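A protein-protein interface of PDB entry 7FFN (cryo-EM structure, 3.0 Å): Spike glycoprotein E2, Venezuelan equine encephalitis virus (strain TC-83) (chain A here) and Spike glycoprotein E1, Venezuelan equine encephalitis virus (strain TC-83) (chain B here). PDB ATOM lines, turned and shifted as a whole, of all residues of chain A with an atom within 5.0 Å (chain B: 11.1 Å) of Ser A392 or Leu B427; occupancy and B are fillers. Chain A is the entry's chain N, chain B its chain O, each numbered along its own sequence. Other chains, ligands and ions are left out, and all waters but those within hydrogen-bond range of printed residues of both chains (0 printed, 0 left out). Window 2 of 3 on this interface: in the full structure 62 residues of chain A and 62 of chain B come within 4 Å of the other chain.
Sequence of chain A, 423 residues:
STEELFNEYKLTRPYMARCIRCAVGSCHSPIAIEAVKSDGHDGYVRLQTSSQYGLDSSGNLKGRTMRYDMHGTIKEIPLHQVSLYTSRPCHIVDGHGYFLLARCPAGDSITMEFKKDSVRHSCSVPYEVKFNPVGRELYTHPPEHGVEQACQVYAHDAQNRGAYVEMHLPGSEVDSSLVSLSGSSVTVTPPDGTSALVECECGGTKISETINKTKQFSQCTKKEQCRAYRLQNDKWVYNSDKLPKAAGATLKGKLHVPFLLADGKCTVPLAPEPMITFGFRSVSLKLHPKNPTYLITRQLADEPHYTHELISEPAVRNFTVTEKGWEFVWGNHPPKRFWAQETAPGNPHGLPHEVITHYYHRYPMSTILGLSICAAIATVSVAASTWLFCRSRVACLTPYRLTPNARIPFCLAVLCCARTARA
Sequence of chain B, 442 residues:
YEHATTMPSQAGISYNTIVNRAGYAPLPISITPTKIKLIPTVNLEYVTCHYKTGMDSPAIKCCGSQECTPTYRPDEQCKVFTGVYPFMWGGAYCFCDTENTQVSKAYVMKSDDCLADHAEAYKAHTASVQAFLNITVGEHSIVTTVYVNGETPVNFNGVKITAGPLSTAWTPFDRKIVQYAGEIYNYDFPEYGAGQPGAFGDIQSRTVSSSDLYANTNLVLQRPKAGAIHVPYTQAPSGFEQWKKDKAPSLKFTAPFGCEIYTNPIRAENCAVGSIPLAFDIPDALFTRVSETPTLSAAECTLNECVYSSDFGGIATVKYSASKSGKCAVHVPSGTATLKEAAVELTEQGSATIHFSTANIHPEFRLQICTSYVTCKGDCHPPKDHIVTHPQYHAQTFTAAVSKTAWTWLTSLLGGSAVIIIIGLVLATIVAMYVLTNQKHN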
ATOM      1  N   LEU A 388      -5.322  14.637  13.324  1.00  0.00           N
ATOM      2  CA  LEU A 388      -4.447  13.925  14.249  1.00  0.00           C
ATOM      3  C   LEU A 388      -4.328  12.445  13.900  1.00  0.00           C
ATOM      4  O   LEU A 388      -3.268  11.847  14.121  1.00  0.00           O
ATOM      5  CB  LEU A 388      -4.945  14.093  15.684  1.00  0.00           C
ATOM      6  CG  LEU A 388      -4.799  15.494  16.274  1.00  0.00           C
ATOM      7  CD1 LEU A 388      -5.471  15.578  17.628  1.00  0.00           C
ATOM      8  CD2 LEU A 388      -3.335  15.850  16.398  1.00  0.00           C
ATOM      9  N   PHE A 389      -5.381  11.853  13.326  1.00  0.00           N
ATOM     10  CA  PHE A 389      -5.296  10.467  12.874  1.00  0.00           C
ATOM     11  C   PHE A 389      -4.328  10.318  11.708  1.00  0.00           C
ATOM     12  O   PHE A 389      -3.521   9.379  11.683  1.00  0.00           O
ATOM     13  CB  PHE A 389      -6.680   9.959  12.479  1.00  0.00           C
ATOM     14  CG  PHE A 389      -6.698   8.523  12.038  1.00  0.00           C
ATOM     15  CD1 PHE A 389      -6.623   7.498  12.968  1.00  0.00           C
ATOM     16  CD2 PHE A 389      -6.798   8.199  10.694  1.00  0.00           C
ATOM     17  CE1 PHE A 389      -6.645   6.174  12.565  1.00  0.00           C
ATOM     18  CE2 PHE A 389      -6.816   6.878  10.284  1.00  0.00           C
ATOM     19  CZ  PHE A 389      -6.740   5.864  11.224  1.00  0.00           C
ATOM     20  N   CYS A 390      -4.396  11.229  10.731  1.00  0.00           N
ATOM     21  CA  CYS A 390      -3.454  11.182   9.613  1.00  0.00           C
ATOM     22  C   CYS A 390      -2.030  11.475  10.073  1.00  0.00           C
ATOM     23  O   CYS A 390      -1.073  10.873   9.565  1.00  0.00           O
ATOM     24  CB  CYS A 390      -3.878  12.159   8.518  1.00  0.00           C
ATOM     25  SG  CYS A 390      -5.381  11.690   7.644  1.00  0.00           S
ATOM     26  N   ARG A 391      -1.878  12.371  11.055  1.00  0.00           N
ATOM     27  CA  ARG A 391      -0.563  12.659  11.623  1.00  0.00           C
ATOM     28  C   ARG A 391       0.028  11.433  12.308  1.00  0.00           C
ATOM     29  O   ARG A 391       1.210  11.120  12.123  1.00  0.00           O
ATOM     30  CB  ARG A 391      -0.680  13.825  12.605  1.00  0.00           C
ATOM     31  CG  ARG A 391       0.614  14.248  13.270  1.00  0.00           C
ATOM     32  CD  ARG A 391       1.575  14.850  12.264  1.00  0.00           C
ATOM     33  NE  ARG A 391       1.034  16.060  11.657  1.00  0.00           N
ATOM     34  CZ  ARG A 391       1.567  16.661  10.598  1.00  0.00           C
ATOM     35  NH1 ARG A 391       2.662  16.168  10.037  1.00  0.00           N
ATOM     36  NH2 ARG A 391       1.011  17.757  10.102  1.00  0.00           N
ATOM     37  N   SER A 392      -0.788  10.699  13.070  1.00  0.00           N
ATOM     38  CA  SER A 392      -0.283   9.505  13.737  1.00  0.00           C
ATOM     39  C   SER A 392      -0.039   8.358  12.764  1.00  0.00           C
ATOM     40  O   SER A 392       0.864   7.549  12.993  1.00  0.00           O
ATOM     41  CB  SER A 392      -1.239   9.066  14.841  1.00  0.00           C
ATOM     42  OG  SER A 392      -1.272  10.018  15.887  1.00  0.00           O
ATOM     43  N   ARG A 393      -0.801   8.279  11.672  1.00  0.00           N
ATOM     44  CA  ARG A 393      -0.529   7.244  10.675  1.00  0.00           C
ATOM     45  C   ARG A 393       0.779   7.516   9.938  1.00  0.00           C
ATOM     46  O   ARG A 393       1.554   6.583   9.673  1.00  0.00           O
ATOM     47  CB  ARG A 393      -1.686   7.138   9.683  1.00  0.00           C
ATOM     48  CG  ARG A 393      -1.516   6.008   8.684  1.00  0.00           C
ATOM     49  CD  ARG A 393      -2.668   5.928   7.715  1.00  0.00           C
ATOM     50  NE  ARG A 393      -2.485   4.845   6.757  1.00  0.00           N
ATOM     51  CZ  ARG A 393      -1.850   4.978   5.599  1.00  0.00           C
ATOM     52  NH1 ARG A 393      -1.336   6.149   5.255  1.00  0.00           N
ATOM     53  NH2 ARG A 393      -1.733   3.942   4.782  1.00  0.00           N
ATOM     54  N   VAL A 394       1.047   8.787   9.613  1.00  0.00           N
ATOM     55  CA  VAL A 394       2.337   9.156   9.038  1.00  0.00           C
ATOM     56  C   VAL A 394       3.466   8.873  10.023  1.00  0.00           C
ATOM     57  O   VAL A 394       4.501   8.310   9.651  1.00  0.00           O
ATOM     58  CB  VAL A 394       2.324  10.629   8.585  1.00  0.00           C
ATOM     59  CG1 VAL A 394       3.719  11.102   8.206  1.00  0.00           C
ATOM     60  CG2 VAL A 394       1.401  10.800   7.396  1.00  0.00           C
ATOM     61  N   ALA A 395       3.259   9.200  11.304  1.00  0.00           N
ATOM     62  CA  ALA A 395       4.297   8.977  12.306  1.00  0.00           C
ATOM     63  C   ALA A 395       4.541   7.494  12.568  1.00  0.00           C
ATOM     64  O   ALA A 395       5.652   7.114  12.948  1.00  0.00           O
ATOM     65  CB  ALA A 395       3.930   9.691  13.607  1.00  0.00           C
ATOM     66  N   CYS A 396       3.530   6.647  12.371  1.00  0.00           N
ATOM     67  CA  CYS A 396       3.762   5.207  12.423  1.00  0.00           C
ATOM     68  C   CYS A 396       4.558   4.735  11.217  1.00  0.00           C
ATOM     69  O   CYS A 396       5.551   4.016  11.363  1.00  0.00           O
ATOM     70  CB  CYS A 396       2.441   4.444  12.502  1.00  0.00           C
ATOM     71  SG  CYS A 396       1.596   4.527  14.087  1.00  0.00           S
ATOM     72  N   ALA B 418     -16.053  16.259  22.196  1.00  0.00           N
ATOM     73  CA  ALA B 418     -14.951  16.320  23.151  1.00  0.00           C
ATOM     74  C   ALA B 418     -14.360  14.940  23.401  1.00  0.00           C
ATOM     75  O   ALA B 418     -13.144  14.803  23.570  1.00  0.00           O
ATOM     76  CB  ALA B 418     -15.426  16.948  24.460  1.00  0.00           C
ATOM     77  N   VAL B 419     -15.206  13.906  23.405  1.00  0.00           N
ATOM     78  CA  VAL B 419     -14.720  12.533  23.547  1.00  0.00           C
ATOM     79  C   VAL B 419     -13.855  12.142  22.352  1.00  0.00           C
ATOM     80  O   VAL B 419     -12.779  11.544  22.514  1.00  0.00           O
ATOM     81  CB  VAL B 419     -15.909  11.569  23.740  1.00  0.00           C
ATOM     82  CG1 VAL B 419     -15.456  10.123  23.696  1.00  0.00           C
ATOM     83  CG2 VAL B 419     -16.578  11.841  25.076  1.00  0.00           C
ATOM     84  N   ILE B 420     -14.282  12.517  21.144  1.00  0.00           N
ATOM     85  CA  ILE B 420     -13.511  12.204  19.942  1.00  0.00           C
ATOM     86  C   ILE B 420     -12.180  12.958  19.933  1.00  0.00           C
ATOM     87  O   ILE B 420     -11.136  12.391  19.582  1.00  0.00           O
ATOM     88  CB  ILE B 420     -14.349  12.490  18.680  1.00  0.00           C
ATOM     89  CG1 ILE B 420     -15.536  11.534  18.603  1.00  0.00           C
ATOM     90  CG2 ILE B 420     -13.547  12.296  17.422  1.00  0.00           C
ATOM     91  CD1 ILE B 420     -16.526  11.906  17.531  1.00  0.00           C
ATOM     92  N   ILE B 421     -12.172  14.219  20.378  1.00  0.00           N
ATOM     93  CA  ILE B 421     -10.906  14.951  20.347  1.00  0.00           C
ATOM     94  C   ILE B 421      -9.961  14.476  21.455  1.00  0.00           C
ATOM     95  O   ILE B 421      -8.738  14.434  21.249  1.00  0.00           O
ATOM     96  CB  ILE B 421     -11.140  16.481  20.367  1.00  0.00           C
ATOM     97  CG1 ILE B 421      -9.866  17.222  19.959  1.00  0.00           C
ATOM     98  CG2 ILE B 421     -11.587  16.996  21.717  1.00  0.00           C
ATOM     99  CD1 ILE B 421      -9.465  16.988  18.527  1.00  0.00           C
ATOM    100  N   ILE B 422     -10.482  14.019  22.601  1.00  0.00           N
ATOM    101  CA  ILE B 422      -9.544  13.548  23.615  1.00  0.00           C
ATOM    102  C   ILE B 422      -9.037  12.147  23.288  1.00  0.00           C
ATOM    103  O   ILE B 422      -7.894  11.814  23.622  1.00  0.00           O
ATOM    104  CB  ILE B 422     -10.120  13.613  25.041  1.00  0.00           C
ATOM    105  CG1 ILE B 422     -11.319  12.684  25.225  1.00  0.00           C
ATOM    106  CG2 ILE B 422     -10.446  15.048  25.426  1.00  0.00           C
ATOM    107  CD1 ILE B 422     -11.751  12.534  26.666  1.00  0.00           C
ATOM    108  N   ILE B 423      -9.824  11.312  22.600  1.00  0.00           N
ATOM    109  CA  ILE B 423      -9.243  10.042  22.176  1.00  0.00           C
ATOM    110  C   ILE B 423      -8.297  10.238  20.997  1.00  0.00           C
ATOM    111  O   ILE B 423      -7.362   9.447  20.835  1.00  0.00           O
ATOM    112  CB  ILE B 423     -10.299   8.968  21.853  1.00  0.00           C
ATOM    113  CG1 ILE B 423     -11.143   9.331  20.635  1.00  0.00           C
ATOM    114  CG2 ILE B 423     -11.177   8.710  23.072  1.00  0.00           C
ATOM    115  CD1 ILE B 423     -12.006   8.188  20.129  1.00  0.00           C
ATOM    116  N   GLY B 424      -8.471  11.307  20.209  1.00  0.00           N
ATOM    117  CA  GLY B 424      -7.442  11.671  19.246  1.00  0.00           C
ATOM    118  C   GLY B 424      -6.145  12.098  19.911  1.00  0.00           C
ATOM    119  O   GLY B 424      -5.056  11.735  19.453  1.00  0.00           O
ATOM    120  N   LEU B 425      -6.245  12.849  21.017  1.00  0.00           N
ATOM    121  CA  LEU B 425      -5.049  13.231  21.768  1.00  0.00           C
ATOM    122  C   LEU B 425      -4.358  12.023  22.399  1.00  0.00           C
ATOM    123  O   LEU B 425      -3.124  11.922  22.365  1.00  0.00           O
ATOM    124  CB  LEU B 425      -5.400  14.262  22.841  1.00  0.00           C
ATOM    125  CG  LEU B 425      -5.201  15.753  22.529  1.00  0.00           C
ATOM    126  CD1 LEU B 425      -3.723  16.051  22.362  1.00  0.00           C
ATOM    127  CD2 LEU B 425      -5.962  16.210  21.301  1.00  0.00           C
ATOM    128  N   VAL B 426      -5.135  11.091  22.959  1.00  0.00           N
ATOM    129  CA  VAL B 426      -4.554   9.899  23.573  1.00  0.00           C
ATOM    130  C   VAL B 426      -3.922   8.996  22.516  1.00  0.00           C
ATOM    131  O   VAL B 426      -2.830   8.451  22.725  1.00  0.00           O
ATOM    132  CB  VAL B 426      -5.621   9.167  24.413  1.00  0.00           C
ATOM    133  CG1 VAL B 426      -5.126   7.811  24.904  1.00  0.00           C
ATOM    134  CG2 VAL B 426      -5.999  10.020  25.607  1.00  0.00           C
ATOM    135  N   LEU B 427      -4.562   8.874  21.347  1.00  0.00           N
ATOM    136  CA  LEU B 427      -3.997   8.095  20.246  1.00  0.00           C
ATOM    137  C   LEU B 427      -2.703   8.716  19.725  1.00  0.00           C
ATOM    138  O   LEU B 427      -1.730   7.995  19.465  1.00  0.00           O
ATOM    139  CB  LEU B 427      -5.045   7.960  19.134  1.00  0.00           C
ATOM    140  CG  LEU B 427      -4.898   7.065  17.894  1.00  0.00           C
ATOM    141  CD1 LEU B 427      -4.155   7.739  16.748  1.00  0.00           C
ATOM    142  CD2 LEU B 427      -4.222   5.750  18.266  1.00  0.00           C
ATOM    143  N   ALA B 428      -2.663  10.047  19.598  1.00  0.00           N
ATOM    144  CA  ALA B 428      -1.445  10.714  19.142  1.00  0.00           C
ATOM    145  C   ALA B 428      -0.321  10.576  20.162  1.00  0.00           C
ATOM    146  O   ALA B 428       0.843  10.383  19.785  1.00  0.00           O
ATOM    147  CB  ALA B 428      -1.729  12.185  18.855  1.00  0.00           C
ATOM    148  N   THR B 429      -0.658  10.624  21.453  1.00  0.00           N
ATOM    149  CA  THR B 429       0.348  10.465  22.499  1.00  0.00           C
ATOM    150  C   THR B 429       0.914   9.047  22.518  1.00  0.00           C
ATOM    151  O   THR B 429       2.132   8.861  22.648  1.00  0.00           O
ATOM    152  CB  THR B 429      -0.262  10.831  23.853  1.00  0.00           C
ATOM    153  OG1 THR B 429      -0.760  12.175  23.794  1.00  0.00           O
ATOM    154  CG2 THR B 429       0.768  10.741  24.966  1.00  0.00           C
ATOM    155  N   ILE B 430       0.053   8.039  22.348  1.00  0.00           N
ATOM    156  CA  ILE B 430       0.505   6.648  22.331  1.00  0.00           C
ATOM    157  C   ILE B 430       1.369   6.370  21.100  1.00  0.00           C
ATOM    158  O   ILE B 430       2.399   5.688  21.195  1.00  0.00           O
ATOM    159  CB  ILE B 430      -0.706   5.699  22.432  1.00  0.00           C
ATOM    160  CG1 ILE B 430      -1.316   5.774  23.831  1.00  0.00           C
ATOM    161  CG2 ILE B 430      -0.337   4.260  22.117  1.00  0.00           C
ATOM    162  CD1 ILE B 430      -2.641   5.059  23.959  1.00  0.00           C
ATOM    163  N   VAL B 431       1.001   6.938  19.944  1.00  0.00           N
ATOM    164  CA  VAL B 431       1.813   6.765  18.737  1.00  0.00           C
ATOM    165  C   VAL B 431       3.174   7.445  18.887  1.00  0.00           C
ATOM    166  O   VAL B 431       4.210   6.865  18.528  1.00  0.00           O
ATOM    167  CB  VAL B 431       1.039   7.272  17.505  1.00  0.00           C
ATOM    168  CG1 VAL B 431       1.948   7.400  16.296  1.00  0.00           C
ATOM    169  CG2 VAL B 431      -0.088   6.310  17.179  1.00  0.00           C
ATOM    170  N   ALA B 432       3.201   8.653  19.466  1.00  0.00           N
ATOM    171  CA  ALA B 432       4.468   9.353  19.672  1.00  0.00           C
ATOM    172  C   ALA B 432       5.373   8.609  20.647  1.00  0.00           C
ATOM    173  O   ALA B 432       6.580   8.478  20.405  1.00  0.00           O
ATOM    174  CB  ALA B 432       4.207  10.774  20.168  1.00  0.00           C
ATOM    175  N   MET B 433       4.801   8.071  21.729  1.00  0.00           N
ATOM    176  CA  MET B 433       5.604   7.337  22.703  1.00  0.00           C
ATOM    177  C   MET B 433       6.107   6.016  22.136  1.00  0.00           C
ATOM    178  O   MET B 433       7.241   5.622  22.409  1.00  0.00           O
ATOM    179  CB  MET B 433       4.811   7.103  23.987  1.00  0.00           C
ATOM    180  CG  MET B 433       4.578   8.364  24.795  1.00  0.00           C
ATOM    181  SD  MET B 433       6.139   9.087  25.331  1.00  0.00           S
ATOM    182  CE  MET B 433       5.576  10.641  26.015  1.00  0.00           C
ATOM    183  N   TYR B 434       5.294   5.337  21.320  1.00  0.00           N
ATOM    184  CA  TYR B 434       5.723   4.077  20.719  1.00  0.00           C
ATOM    185  C   TYR B 434       6.847   4.285  19.712  1.00  0.00           C
ATOM    186  O   TYR B 434       7.838   3.536  19.712  1.00  0.00           O
ATOM    187  CB  TYR B 434       4.524   3.394  20.063  1.00  0.00           C
ATOM    188  CG  TYR B 434       4.831   2.076  19.398  1.00  0.00           C
ATOM    189  CD1 TYR B 434       5.065   0.932  20.154  1.00  0.00           C
ATOM    190  CD2 TYR B 434       4.866   1.968  18.012  1.00  0.00           C
ATOM    191  CE1 TYR B 434       5.337  -0.279  19.547  1.00  0.00           C
ATOM    192  CE2 TYR B 434       5.136   0.760  17.396  1.00  0.00           C
ATOM    193  CZ  TYR B 434       5.373  -0.357  18.168  1.00  0.00           C
ATOM    194  OH  TYR B 434       5.642  -1.562  17.560  1.00  0.00           O
ATOM    195  N   VAL B 435       6.727   5.316  18.869  1.00  0.00           N
ATOM    196  CA  VAL B 435       7.751   5.584  17.862  1.00  0.00           C
ATOM    197  C   VAL B 435       9.034   6.091  18.514  1.00  0.00           C
ATOM    198  O   VAL B 435      10.142   5.728  18.094  1.00  0.00           O
ATOM    199  CB  VAL B 435       7.195   6.557  16.804  1.00  0.00           C
ATOM    200  CG1 VAL B 435       8.270   7.013  15.827  1.00  0.00           C
ATOM    201  CG2 VAL B 435       6.080   5.880  16.032  1.00  0.00           C
ATOM    202  N   LEU B 436       8.920   6.880  19.584  1.00  0.00           N
ATOM    203  CA  LEU B 436      10.125   7.287  20.300  1.00  0.00           C
ATOM    204  C   LEU B 436      10.725   6.132  21.101  1.00  0.00           C
ATOM    205  O   LEU B 436      11.939   6.110  21.333  1.00  0.00           O
ATOM    206  CB  LEU B 436       9.806   8.486  21.198  1.00  0.00           C
ATOM    207  CG  LEU B 436      10.925   9.286  21.868  1.00  0.00           C
ATOM    208  CD1 LEU B 436      10.524  10.742  21.919  1.00  0.00           C
ATOM    209  CD2 LEU B 436      11.208   8.793  23.280  1.00  0.00           C
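O of Ser A392 sits at hydrogen-bond distance from SG of Cys A396 (3.3 Å). O of Leu A388 is in hydrogen-bond range of OG of Ser A392, at 3.2 Å. The backbone carbonyl oxygen (O) of Leu B425 sits at hydrogen-bond distance from the side-chain hydroxyl (OG1) of Thr B429 (2.8 Å).
Among the printed residues, pairs that only touch across the chains: Leu A388 with Leu B425 (3.8 Å), Ser A392 with Leu B427 (3.7 Å), Ser A392 with Ala B428 (3.3 Å), Ser A392 with Val B431 (3.5 Å), Ala A395 with Val B435 (3.3 Å) and Cys A396 with Val B431 (3.6 Å).
Of the 19 printed residues of chain B, 5 touch a printed residue of chain A. Hydrophobic or aromatic side chains of chain B that line the printed part of chain A: Leu B425, Leu B427, Ala B428, Val B431 and Val B435. Hydrophobic or aromatic side chains of chain A within 4 Å of the printed part of chain B: Leu A388. Along chain A the printed residues that touch a printed residue of chain B span positions 388 to 396. Among the printed residues, 6 pairs touch across the chains.
Of chain B, only Leu B427, Ala B428 and Val B431 come within 4 Å of Ser A392. Leu B427 touches just one residue of chain A: Ser A392 (3.7 Å). No residue of chain B comes within 4 Å of Phe A389. No residue of chain B comes within 4 Å of Val A394. Of chain B, only Val B435 comes within 4 Å of Ala A395. Cys A396 touches just one residue of chain B: Val B431. Of the printed residues of chain A, Leu B425 touches Leu A388 (3.8 Å). Printed residues of chain B within 4 Å of Leu A388: Leu B425 (3.8 Å). Of the printed residues of chain A, Val B431 touches Ser A392 and Cys A396. Of the printed residues of chain A, Ala B428 touches Ser A392. Of the printed residues of chain A, Val B435 touches Ala A395 (3.3 Å). Val B426 touches none of the printed residues of chain A. The nearest printed residue of chain A that does not touch Val B431 is Ala A395 (4.1 Å).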
